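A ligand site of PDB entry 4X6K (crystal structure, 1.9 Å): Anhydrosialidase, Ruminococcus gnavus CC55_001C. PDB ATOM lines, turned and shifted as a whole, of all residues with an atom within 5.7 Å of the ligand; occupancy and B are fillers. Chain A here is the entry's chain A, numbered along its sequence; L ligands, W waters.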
ATOM      1  N   ARG A  20      -0.928 -12.806 -22.337  1.00  0.00           N
ATOM      2  CA  ARG A  20      -2.004 -11.848 -22.313  1.00  0.00           C
ATOM      3  C   ARG A  20      -1.396 -10.488 -22.703  1.00  0.00           C
ATOM      4  O   ARG A  20      -0.193 -10.344 -22.635  1.00  0.00           O
ATOM      5  CB  ARG A  20      -2.661 -11.685 -20.915  1.00  0.00           C
ATOM      6  CG  ARG A  20      -3.774 -12.668 -20.662  1.00  0.00           C
ATOM      7  CD  ARG A  20      -4.645 -12.172 -19.545  1.00  0.00           C
ATOM      8  NE  ARG A  20      -5.329 -10.969 -20.033  1.00  0.00           N
ATOM      9  CZ  ARG A  20      -5.935 -10.098 -19.268  1.00  0.00           C
ATOM     10  NH1 ARG A  20      -6.121 -10.371 -17.979  1.00  0.00           N
ATOM     11  NH2 ARG A  20      -6.447  -8.986 -19.826  1.00  0.00           N
ATOM     12  N   ILE A  21      -2.271  -9.527 -23.087  1.00  0.00           N
ATOM     13  CA  ILE A  21      -1.987  -8.084 -23.176  1.00  0.00           C
ATOM     14  C   ILE A  21      -1.122  -7.810 -24.427  1.00  0.00           C
ATOM     15  O   ILE A  21       0.049  -7.456 -24.342  1.00  0.00           O
ATOM     16  CB  ILE A  21      -1.273  -7.487 -21.973  1.00  0.00           C
ATOM     17  CG1 ILE A  21      -1.736  -8.075 -20.591  1.00  0.00           C
ATOM     18  CG2 ILE A  21      -1.468  -5.977 -21.999  1.00  0.00           C
ATOM     19  CD1 ILE A  21      -3.237  -7.916 -20.319  1.00  0.00           C
ATOM     20  N   ASP A  37       2.615  -9.935 -22.256  1.00  0.00           N
ATOM     21  CA  ASP A  37       2.984 -10.558 -21.023  1.00  0.00           C
ATOM     22  C   ASP A  37       3.271 -12.069 -21.250  1.00  0.00           C
ATOM     23  O   ASP A  37       2.429 -12.814 -21.812  1.00  0.00           O
ATOM     24  CB  ASP A  37       1.853 -10.544 -19.958  1.00  0.00           C
ATOM     25  CG  ASP A  37       1.656  -9.232 -19.268  1.00  0.00           C
ATOM     26  OD1 ASP A  37       2.292  -8.165 -19.548  1.00  0.00           O
ATOM     27  OD2 ASP A  37       0.737  -9.279 -18.416  1.00  0.00           O
ATOM     28  N   ARG A  39       2.990 -14.845 -19.040  1.00  0.00           N
ATOM     29  CA  ARG A  39       2.397 -15.074 -17.721  1.00  0.00           C
ATOM     30  C   ARG A  39       2.655 -16.569 -17.349  1.00  0.00           C
ATOM     31  O   ARG A  39       2.023 -17.466 -17.863  1.00  0.00           O
ATOM     32  CB  ARG A  39       0.924 -14.761 -17.681  1.00  0.00           C
ATOM     33  CG  ARG A  39       0.589 -13.279 -17.832  1.00  0.00           C
ATOM     34  CD  ARG A  39      -0.788 -12.893 -17.387  1.00  0.00           C
ATOM     35  NE  ARG A  39      -0.928 -11.474 -17.516  1.00  0.00           N
ATOM     36  CZ  ARG A  39      -1.909 -10.725 -17.009  1.00  0.00           C
ATOM     37  NH1 ARG A  39      -2.852 -11.268 -16.263  1.00  0.00           N
ATOM     38  NH2 ARG A  39      -1.872  -9.407 -17.157  1.00  0.00           N
ATOM     39  N   ASP A  45      -2.996 -11.740 -13.027  1.00  0.00           N
ATOM     40  CA  ASP A  45      -2.328 -10.459 -12.843  1.00  0.00           C
ATOM     41  C   ASP A  45      -1.273 -10.578 -11.756  1.00  0.00           C
ATOM     42  O   ASP A  45      -1.355 -11.462 -10.936  1.00  0.00           O
ATOM     43  CB  ASP A  45      -3.301  -9.391 -12.456  1.00  0.00           C
ATOM     44  CG  ASP A  45      -4.320  -9.090 -13.530  1.00  0.00           C
ATOM     45  OD1 ASP A  45      -4.061  -9.367 -14.773  1.00  0.00           O
ATOM     46  OD2 ASP A  45      -5.295  -8.413 -13.141  1.00  0.00           O
ATOM     47  N   ALA A  46      -0.278  -9.702 -11.772  1.00  0.00           N
ATOM     48  CA  ALA A  46       0.515  -9.571 -10.620  1.00  0.00           C
ATOM     49  C   ALA A  46      -0.408  -9.308  -9.373  1.00  0.00           C
ATOM     50  O   ALA A  46      -1.431  -8.568  -9.467  1.00  0.00           O
ATOM     51  CB  ALA A  46       1.559  -8.469 -10.819  1.00  0.00           C
ATOM     52  N   ILE A 101       4.485  -6.317 -16.291  1.00  0.00           N
ATOM     53  CA  ILE A 101       3.114  -6.570 -16.649  1.00  0.00           C
ATOM     54  C   ILE A 101       2.616  -5.349 -17.432  1.00  0.00           C
ATOM     55  O   ILE A 101       2.943  -4.209 -17.077  1.00  0.00           O
ATOM     56  CB  ILE A 101       2.226  -6.887 -15.412  1.00  0.00           C
ATOM     57  CG1 ILE A 101       0.720  -6.958 -15.737  1.00  0.00           C
ATOM     58  CG2 ILE A 101       2.423  -5.834 -14.311  1.00  0.00           C
ATOM     59  CD1 ILE A 101      -0.202  -7.612 -14.688  1.00  0.00           C
ATOM     60  N   ASP A 102       1.868  -5.628 -18.503  1.00  0.00           N
ATOM     61  CA  ASP A 102       1.026  -4.646 -19.250  1.00  0.00           C
ATOM     62  C   ASP A 102       1.926  -3.750 -20.129  1.00  0.00           C
ATOM     63  O   ASP A 102       2.127  -2.590 -19.835  1.00  0.00           O
ATOM     64  CB  ASP A 102       0.130  -3.792 -18.324  1.00  0.00           C
ATOM     65  CG  ASP A 102      -1.192  -4.447 -17.969  1.00  0.00           C
ATOM     66  OD1 ASP A 102      -1.377  -5.634 -18.224  1.00  0.00           O
ATOM     67  OD2 ASP A 102      -2.020  -3.779 -17.254  1.00  0.00           O
ATOM     68  N   ASP A 119       4.735  -2.131 -16.570  1.00  0.00           N
ATOM     69  CA  ASP A 119       4.621  -1.881 -15.140  1.00  0.00           C
ATOM     70  C   ASP A 119       5.638  -2.826 -14.489  1.00  0.00           C
ATOM     71  O   ASP A 119       5.749  -3.957 -14.877  1.00  0.00           O
ATOM     72  CB  ASP A 119       3.222  -2.175 -14.591  1.00  0.00           C
ATOM     73  CG  ASP A 119       2.111  -1.483 -15.331  1.00  0.00           C
ATOM     74  OD1 ASP A 119       2.318  -0.354 -15.882  1.00  0.00           O
ATOM     75  OD2 ASP A 119       0.999  -2.109 -15.326  1.00  0.00           O
ATOM     76  N   MET A 121       6.859  -4.531 -10.879  1.00  0.00           N
ATOM     77  CA  MET A 121       6.231  -4.849  -9.647  1.00  0.00           C
ATOM     78  C   MET A 121       7.247  -5.561  -8.813  1.00  0.00           C
ATOM     79  O   MET A 121       7.734  -6.617  -9.191  1.00  0.00           O
ATOM     80  CB  MET A 121       5.019  -5.751  -9.841  1.00  0.00           C
ATOM     81  CG  MET A 121       3.960  -5.216 -10.760  1.00  0.00           C
ATOM     82  SD  MET A 121       3.055  -3.892  -9.998  1.00  0.00           S
ATOM     83  CE  MET A 121       1.708  -3.813 -11.196  1.00  0.00           C
ATOM     84  N   SER A 127      -1.012  -4.295  -8.600  1.00  0.00           N
ATOM     85  CA  SER A 127      -1.728  -3.077  -8.406  1.00  0.00           C
ATOM     86  C   SER A 127      -2.582  -3.121  -7.179  1.00  0.00           C
ATOM     87  O   SER A 127      -2.577  -2.144  -6.439  1.00  0.00           O
ATOM     88  CB  SER A 127      -2.620  -2.797  -9.606  1.00  0.00           C
ATOM     89  OG  SER A 127      -1.808  -2.336 -10.652  1.00  0.00           O
ATOM     90  N   VAL A 265       0.046   3.181 -13.595  1.00  0.00           N
ATOM     91  CA  VAL A 265       0.401   2.134 -14.492  1.00  0.00           C
ATOM     92  C   VAL A 265       0.055   2.504 -15.939  1.00  0.00           C
ATOM     93  O   VAL A 265      -0.597   3.482 -16.208  1.00  0.00           O
ATOM     94  CB  VAL A 265      -0.340   0.833 -14.103  1.00  0.00           C
ATOM     95  CG1 VAL A 265       0.137   0.293 -12.750  1.00  0.00           C
ATOM     96  CG2 VAL A 265      -1.843   1.034 -14.020  1.00  0.00           C
ATOM     97  N   TYR A 288      -2.793   5.143 -16.208  1.00  0.00           N
ATOM     98  CA  TYR A 288      -3.956   5.367 -15.355  1.00  0.00           C
ATOM     99  C   TYR A 288      -3.585   5.120 -13.930  1.00  0.00           C
ATOM    100  O   TYR A 288      -2.555   4.483 -13.648  1.00  0.00           O
ATOM    101  CB  TYR A 288      -5.232   4.526 -15.765  1.00  0.00           C
ATOM    102  CG  TYR A 288      -5.120   3.012 -15.568  1.00  0.00           C
ATOM    103  CD1 TYR A 288      -4.493   2.180 -16.528  1.00  0.00           C
ATOM    104  CD2 TYR A 288      -5.566   2.428 -14.389  1.00  0.00           C
ATOM    105  CE1 TYR A 288      -4.360   0.847 -16.321  1.00  0.00           C
ATOM    106  CE2 TYR A 288      -5.461   1.077 -14.181  1.00  0.00           C
ATOM    107  CZ  TYR A 288      -4.850   0.287 -15.145  1.00  0.00           C
ATOM    108  OH  TYR A 288      -4.702  -1.029 -14.870  1.00  0.00           O
ATOM    109  N   THR A 320     -10.081   1.357 -14.130  1.00  0.00           N
ATOM    110  CA  THR A 320      -9.066   0.847 -15.089  1.00  0.00           C
ATOM    111  C   THR A 320      -9.210   1.630 -16.426  1.00  0.00           C
ATOM    112  O   THR A 320      -9.614   1.046 -17.447  1.00  0.00           O
ATOM    113  CB  THR A 320      -9.165  -0.673 -15.253  1.00  0.00           C
ATOM    114  OG1 THR A 320      -9.072  -1.298 -13.975  1.00  0.00           O
ATOM    115  CG2 THR A 320      -8.029  -1.239 -16.108  1.00  0.00           C
ATOM    116  N   GLU A 322      -7.682   2.604 -19.083  1.00  0.00           N
ATOM    117  CA  GLU A 322      -6.709   2.309 -20.130  1.00  0.00           C
ATOM    118  C   GLU A 322      -7.124   3.017 -21.376  1.00  0.00           C
ATOM    119  O   GLU A 322      -8.296   2.877 -21.800  1.00  0.00           O
ATOM    120  CB  GLU A 322      -6.774   0.875 -20.426  1.00  0.00           C
ATOM    121  CG  GLU A 322      -6.317  -0.002 -19.259  1.00  0.00           C
ATOM    122  CD  GLU A 322      -6.695  -1.435 -19.392  1.00  0.00           C
ATOM    123  OE1 GLU A 322      -7.814  -1.636 -19.882  1.00  0.00           O
ATOM    124  OE2 GLU A 322      -5.889  -2.400 -19.031  1.00  0.00           O
ATOM    125  N   ARG A 338     -11.106   3.169 -21.787  1.00  0.00           N
ATOM    126  CA  ARG A 338     -11.968   2.333 -21.055  1.00  0.00           C
ATOM    127  C   ARG A 338     -12.398   3.169 -19.841  1.00  0.00           C
ATOM    128  O   ARG A 338     -11.620   3.960 -19.375  1.00  0.00           O
ATOM    129  CB  ARG A 338     -11.103   1.205 -20.520  1.00  0.00           C
ATOM    130  CG  ARG A 338     -11.794   0.250 -19.585  1.00  0.00           C
ATOM    131  CD  ARG A 338     -10.917  -0.990 -19.340  1.00  0.00           C
ATOM    132  NE  ARG A 338     -11.382  -1.863 -18.255  1.00  0.00           N
ATOM    133  CZ  ARG A 338     -10.752  -2.960 -17.828  1.00  0.00           C
ATOM    134  NH1 ARG A 338      -9.652  -3.365 -18.440  1.00  0.00           N
ATOM    135  NH2 ARG A 338     -11.246  -3.649 -16.814  1.00  0.00           N
ATOM    136  N   GLY A 371     -15.476  -2.852 -18.039  1.00  0.00           N
ATOM    137  CA  GLY A 371     -14.829  -2.433 -19.298  1.00  0.00           C
ATOM    138  C   GLY A 371     -13.726  -3.378 -19.771  1.00  0.00           C
ATOM    139  O   GLY A 371     -13.339  -4.312 -19.075  1.00  0.00           O
ATOM    140  N   ARG A 400     -16.690 -10.528 -22.221  1.00  0.00           N
ATOM    141  CA  ARG A 400     -15.778 -10.055 -23.267  1.00  0.00           C
ATOM    142  C   ARG A 400     -15.883 -10.861 -24.518  1.00  0.00           C
ATOM    143  O   ARG A 400     -15.313 -11.924 -24.582  1.00  0.00           O
ATOM    144  CB  ARG A 400     -14.325 -10.078 -22.742  1.00  0.00           C
ATOM    145  CG  ARG A 400     -14.130  -9.043 -21.625  1.00  0.00           C
ATOM    146  CD  ARG A 400     -12.707  -8.913 -21.116  1.00  0.00           C
ATOM    147  NE  ARG A 400     -12.539  -7.741 -20.287  1.00  0.00           N
ATOM    148  CZ  ARG A 400     -11.509  -7.486 -19.470  1.00  0.00           C
ATOM    149  NH1 ARG A 400     -10.522  -8.362 -19.328  1.00  0.00           N
ATOM    150  NH2 ARG A 400     -11.422  -6.304 -18.892  1.00  0.00           N
ATOM    151  N   TYR A 440      -8.511  -8.284 -24.984  1.00  0.00           N
ATOM    152  CA  TYR A 440      -7.573  -7.198 -25.268  1.00  0.00           C
ATOM    153  C   TYR A 440      -7.097  -7.359 -26.698  1.00  0.00           C
ATOM    154  O   TYR A 440      -7.128  -8.490 -27.245  1.00  0.00           O
ATOM    155  CB  TYR A 440      -6.396  -7.251 -24.312  1.00  0.00           C
ATOM    156  CG  TYR A 440      -6.589  -6.598 -22.990  1.00  0.00           C
ATOM    157  CD1 TYR A 440      -7.798  -6.727 -22.289  1.00  0.00           C
ATOM    158  CD2 TYR A 440      -5.586  -5.802 -22.420  1.00  0.00           C
ATOM    159  CE1 TYR A 440      -8.001  -6.102 -21.058  1.00  0.00           C
ATOM    160  CE2 TYR A 440      -5.810  -5.172 -21.191  1.00  0.00           C
ATOM    161  CZ  TYR A 440      -7.025  -5.307 -20.534  1.00  0.00           C
ATOM    162  OH  TYR A 440      -7.293  -4.699 -19.369  1.00  0.00           O
ATOM    163  N   SER A 460     -10.955 -12.798 -20.998  1.00  0.00           N
ATOM    164  CA  SER A 460      -9.894 -12.739 -20.008  1.00  0.00           C
ATOM    165  C   SER A 460     -10.291 -12.144 -18.652  1.00  0.00           C
ATOM    166  O   SER A 460      -9.465 -12.053 -17.771  1.00  0.00           O
ATOM    167  CB  SER A 460      -8.706 -11.981 -20.605  1.00  0.00           C
ATOM    168  OG  SER A 460      -9.054 -10.608 -20.800  1.00  0.00           O
ATOM    169  N   TRP A 461     -11.522 -11.680 -18.507  1.00  0.00           N
ATOM    170  CA  TRP A 461     -12.084 -11.265 -17.207  1.00  0.00           C
ATOM    171  C   TRP A 461     -12.693 -12.468 -16.453  1.00  0.00           C
ATOM    172  O   TRP A 461     -12.568 -12.573 -15.230  1.00  0.00           O
ATOM    173  CB  TRP A 461     -13.175 -10.219 -17.467  1.00  0.00           C
ATOM    174  CG  TRP A 461     -13.742  -9.562 -16.232  1.00  0.00           C
ATOM    175  CD1 TRP A 461     -14.956  -9.836 -15.604  1.00  0.00           C
ATOM    176  CD2 TRP A 461     -13.132  -8.533 -15.467  1.00  0.00           C
ATOM    177  NE1 TRP A 461     -15.099  -9.049 -14.473  1.00  0.00           N
ATOM    178  CE2 TRP A 461     -14.004  -8.225 -14.389  1.00  0.00           C
ATOM    179  CE3 TRP A 461     -11.913  -7.858 -15.557  1.00  0.00           C
ATOM    180  CZ2 TRP A 461     -13.699  -7.246 -13.450  1.00  0.00           C
ATOM    181  CZ3 TRP A 461     -11.629  -6.874 -14.620  1.00  0.00           C
ATOM    182  CH2 TRP A 461     -12.504  -6.570 -13.606  1.00  0.00           C
HETATM  183  C1  LIG L   1      -1.413  -4.131 -13.726  1.00  0.00           C
HETATM  184  C2  LIG L   1      -2.626  -5.002 -13.779  1.00  0.00           C
HETATM  185  O1  LIG L   1      -3.020  -5.681 -12.838  1.00  0.00           O
HETATM  186  N1  LIG L   1      -3.302  -4.884 -14.881  1.00  0.00           N
HETATM  187  C3  LIG L   1      -4.436  -5.678 -15.111  1.00  0.00           C
HETATM  188  N2  LIG L   1      -5.570  -4.709 -14.939  1.00  0.00           N
HETATM  189  C4  LIG L   1      -6.765  -5.530 -15.217  1.00  0.00           C
HETATM  190  C5  LIG L   1      -6.782  -5.920 -16.709  1.00  0.00           C
HETATM  191  C6  LIG L   1      -8.119  -6.445 -17.253  1.00  0.00           C
HETATM  192  O2  LIG L   1      -8.097  -7.467 -18.007  1.00  0.00           O
HETATM  193  O3  LIG L   1      -9.188  -5.756 -16.981  1.00  0.00           O
HETATM  194  C7  LIG L   1      -5.630  -6.928 -16.886  1.00  0.00           C
HETATM  195  O4  LIG L   1      -5.804  -8.017 -16.031  1.00  0.00           O
HETATM  196  C8  LIG L   1      -4.353  -6.166 -16.523  1.00  0.00           C
HETATM  197  O5  LIG L   1      -3.197  -6.968 -16.760  1.00  0.00           O
HETATM  198  O   HOH W   1      -8.797  -9.579 -16.150  1.00  0.00           O
HETATM  199  O   HOH W   2      -1.224  -6.138 -10.828  1.00  0.00           O
HETATM  200  O   HOH W   3      -5.147  -6.772 -11.068  1.00  0.00           O
HETATM  201  O   HOH W   4      -3.854  -2.036 -12.427  1.00  0.00           O
HETATM  202  O   HOH W   5      -4.469  -2.698 -16.963  1.00  0.00           O
HETATM  203  O   HOH W   6      -7.564  -9.101 -13.811  1.00  0.00           O
HETATM  204  O   HOH W   7      -6.186  -4.536 -12.371  1.00  0.00           O
HETATM  205  O   HOH W   8      -8.921  -5.510 -12.510  1.00  0.00           O
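Residues that only touch the ligand: Asp 119 (3.5 Å), Trp 461 (3.6 Å), Ser 127 (3.6 Å), Ile 101 (3.7 Å), Ile 21 (3.7 Å) and Tyr 288 (3.8 Å). Hydrophobic or aromatic side chains within 4 Å of the ligand: Ile 21, Ile 101, Tyr 440 and Trp 461. 13 residues have an atom within 4 Å of the ligand: Arg 20, Ile 21, Arg 39, Asp 45, Ile 101, Asp 102, Asp 119, Ser 127, Tyr 288, Arg 338, Arg 400, Tyr 440 and Trp 461.
The side-chain hydroxyl of Tyr 440 sits at hydrogen-bond distance from the side-chain carboxylate of Glu 322 (2.7 Å). The side-chain carboxylate (OD1) of Asp 45 is in salt-bridge range of the guanidinium group (NH1) of Arg 39, 2.7 Å away. OD1 of Asp 102 lies within salt-bridge range of NH2 of Arg 39 (3.95 Å). The guanidinium group of Arg 338 sits at hydrogen-bond distance from the side-chain hydroxyl of Tyr 440, at 2.9 Å. N of Asp 37 sits at hydrogen-bond distance from O of Arg 20 (2.9 Å). NH2 of Arg 20 sits at hydrogen-bond distance from OG of Ser 460, at 3.2 Å. The guanidinium group (NH1) of Arg 400 lies within hydrogen-bond range of the side-chain hydroxyl (OG) of Ser 460 (3.1 Å). The side-chain carboxylate of Asp 45 is in salt-bridge range of the guanidinium group of Arg 20, at 3.9 Å.
Water W2 lies within hydrogen-bond range of O1 of the ligand (2.7 Å), O of Ala 46 (2.8 Å) and N of Ser 127 (2.9 Å). Water W1 lies within hydrogen-bond range of an oxygen (O2) of the ligand (2.9 Å), the backbone carbonyl oxygen of Ser 460 (3.0 Å) and the guanidinium group of Arg 20 (3.3 Å). Water W3 lies within hydrogen-bond range of OD2 of Asp 45 (2.6 Å) and O1 of the ligand (3.0 Å). Water W6 lies within hydrogen-bond range of the side-chain carboxylate (OD2) of Asp 45 (2.5 Å) and an oxygen (O4) of the ligand (3.0 Å). Water W5 lies within hydrogen-bond range of OE2 of Glu 322 (2.5 Å), OH of Tyr 288 (2.7 Å), OD2 of Asp 102 (2.7 Å) and N2 of the ligand (3.1 Å). Water W4 bridges the side-chain hydroxyl (OG) of Ser 127 (2.7 Å) and the side-chain hydroxyl (OH) of Tyr 288 (2.8 Å).
An oxygen (O2) of the ligand lies within salt-bridge range of the guanidinium group of Arg 20, at 2.9 Å. The side-chain carboxylate (OD1) of Asp 45 sits at hydrogen-bond distance from an oxygen (O4) of the ligand. O2 of the ligand is in salt-bridge range of NH1 of Arg 400 (2.9 Å). O5 of the ligand sits at hydrogen-bond distance from OD1 of Asp 102, 2.7 Å away. NH1 of Arg 338 is in salt-bridge range of O3 of the ligand (2.8 Å). The guanidinium group of Arg 39 lies within hydrogen-bond range of an oxygen (O5) of the ligand (2.8 Å). O2 of the ligand lies close to OH of Tyr 440, at 3.2 Å.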
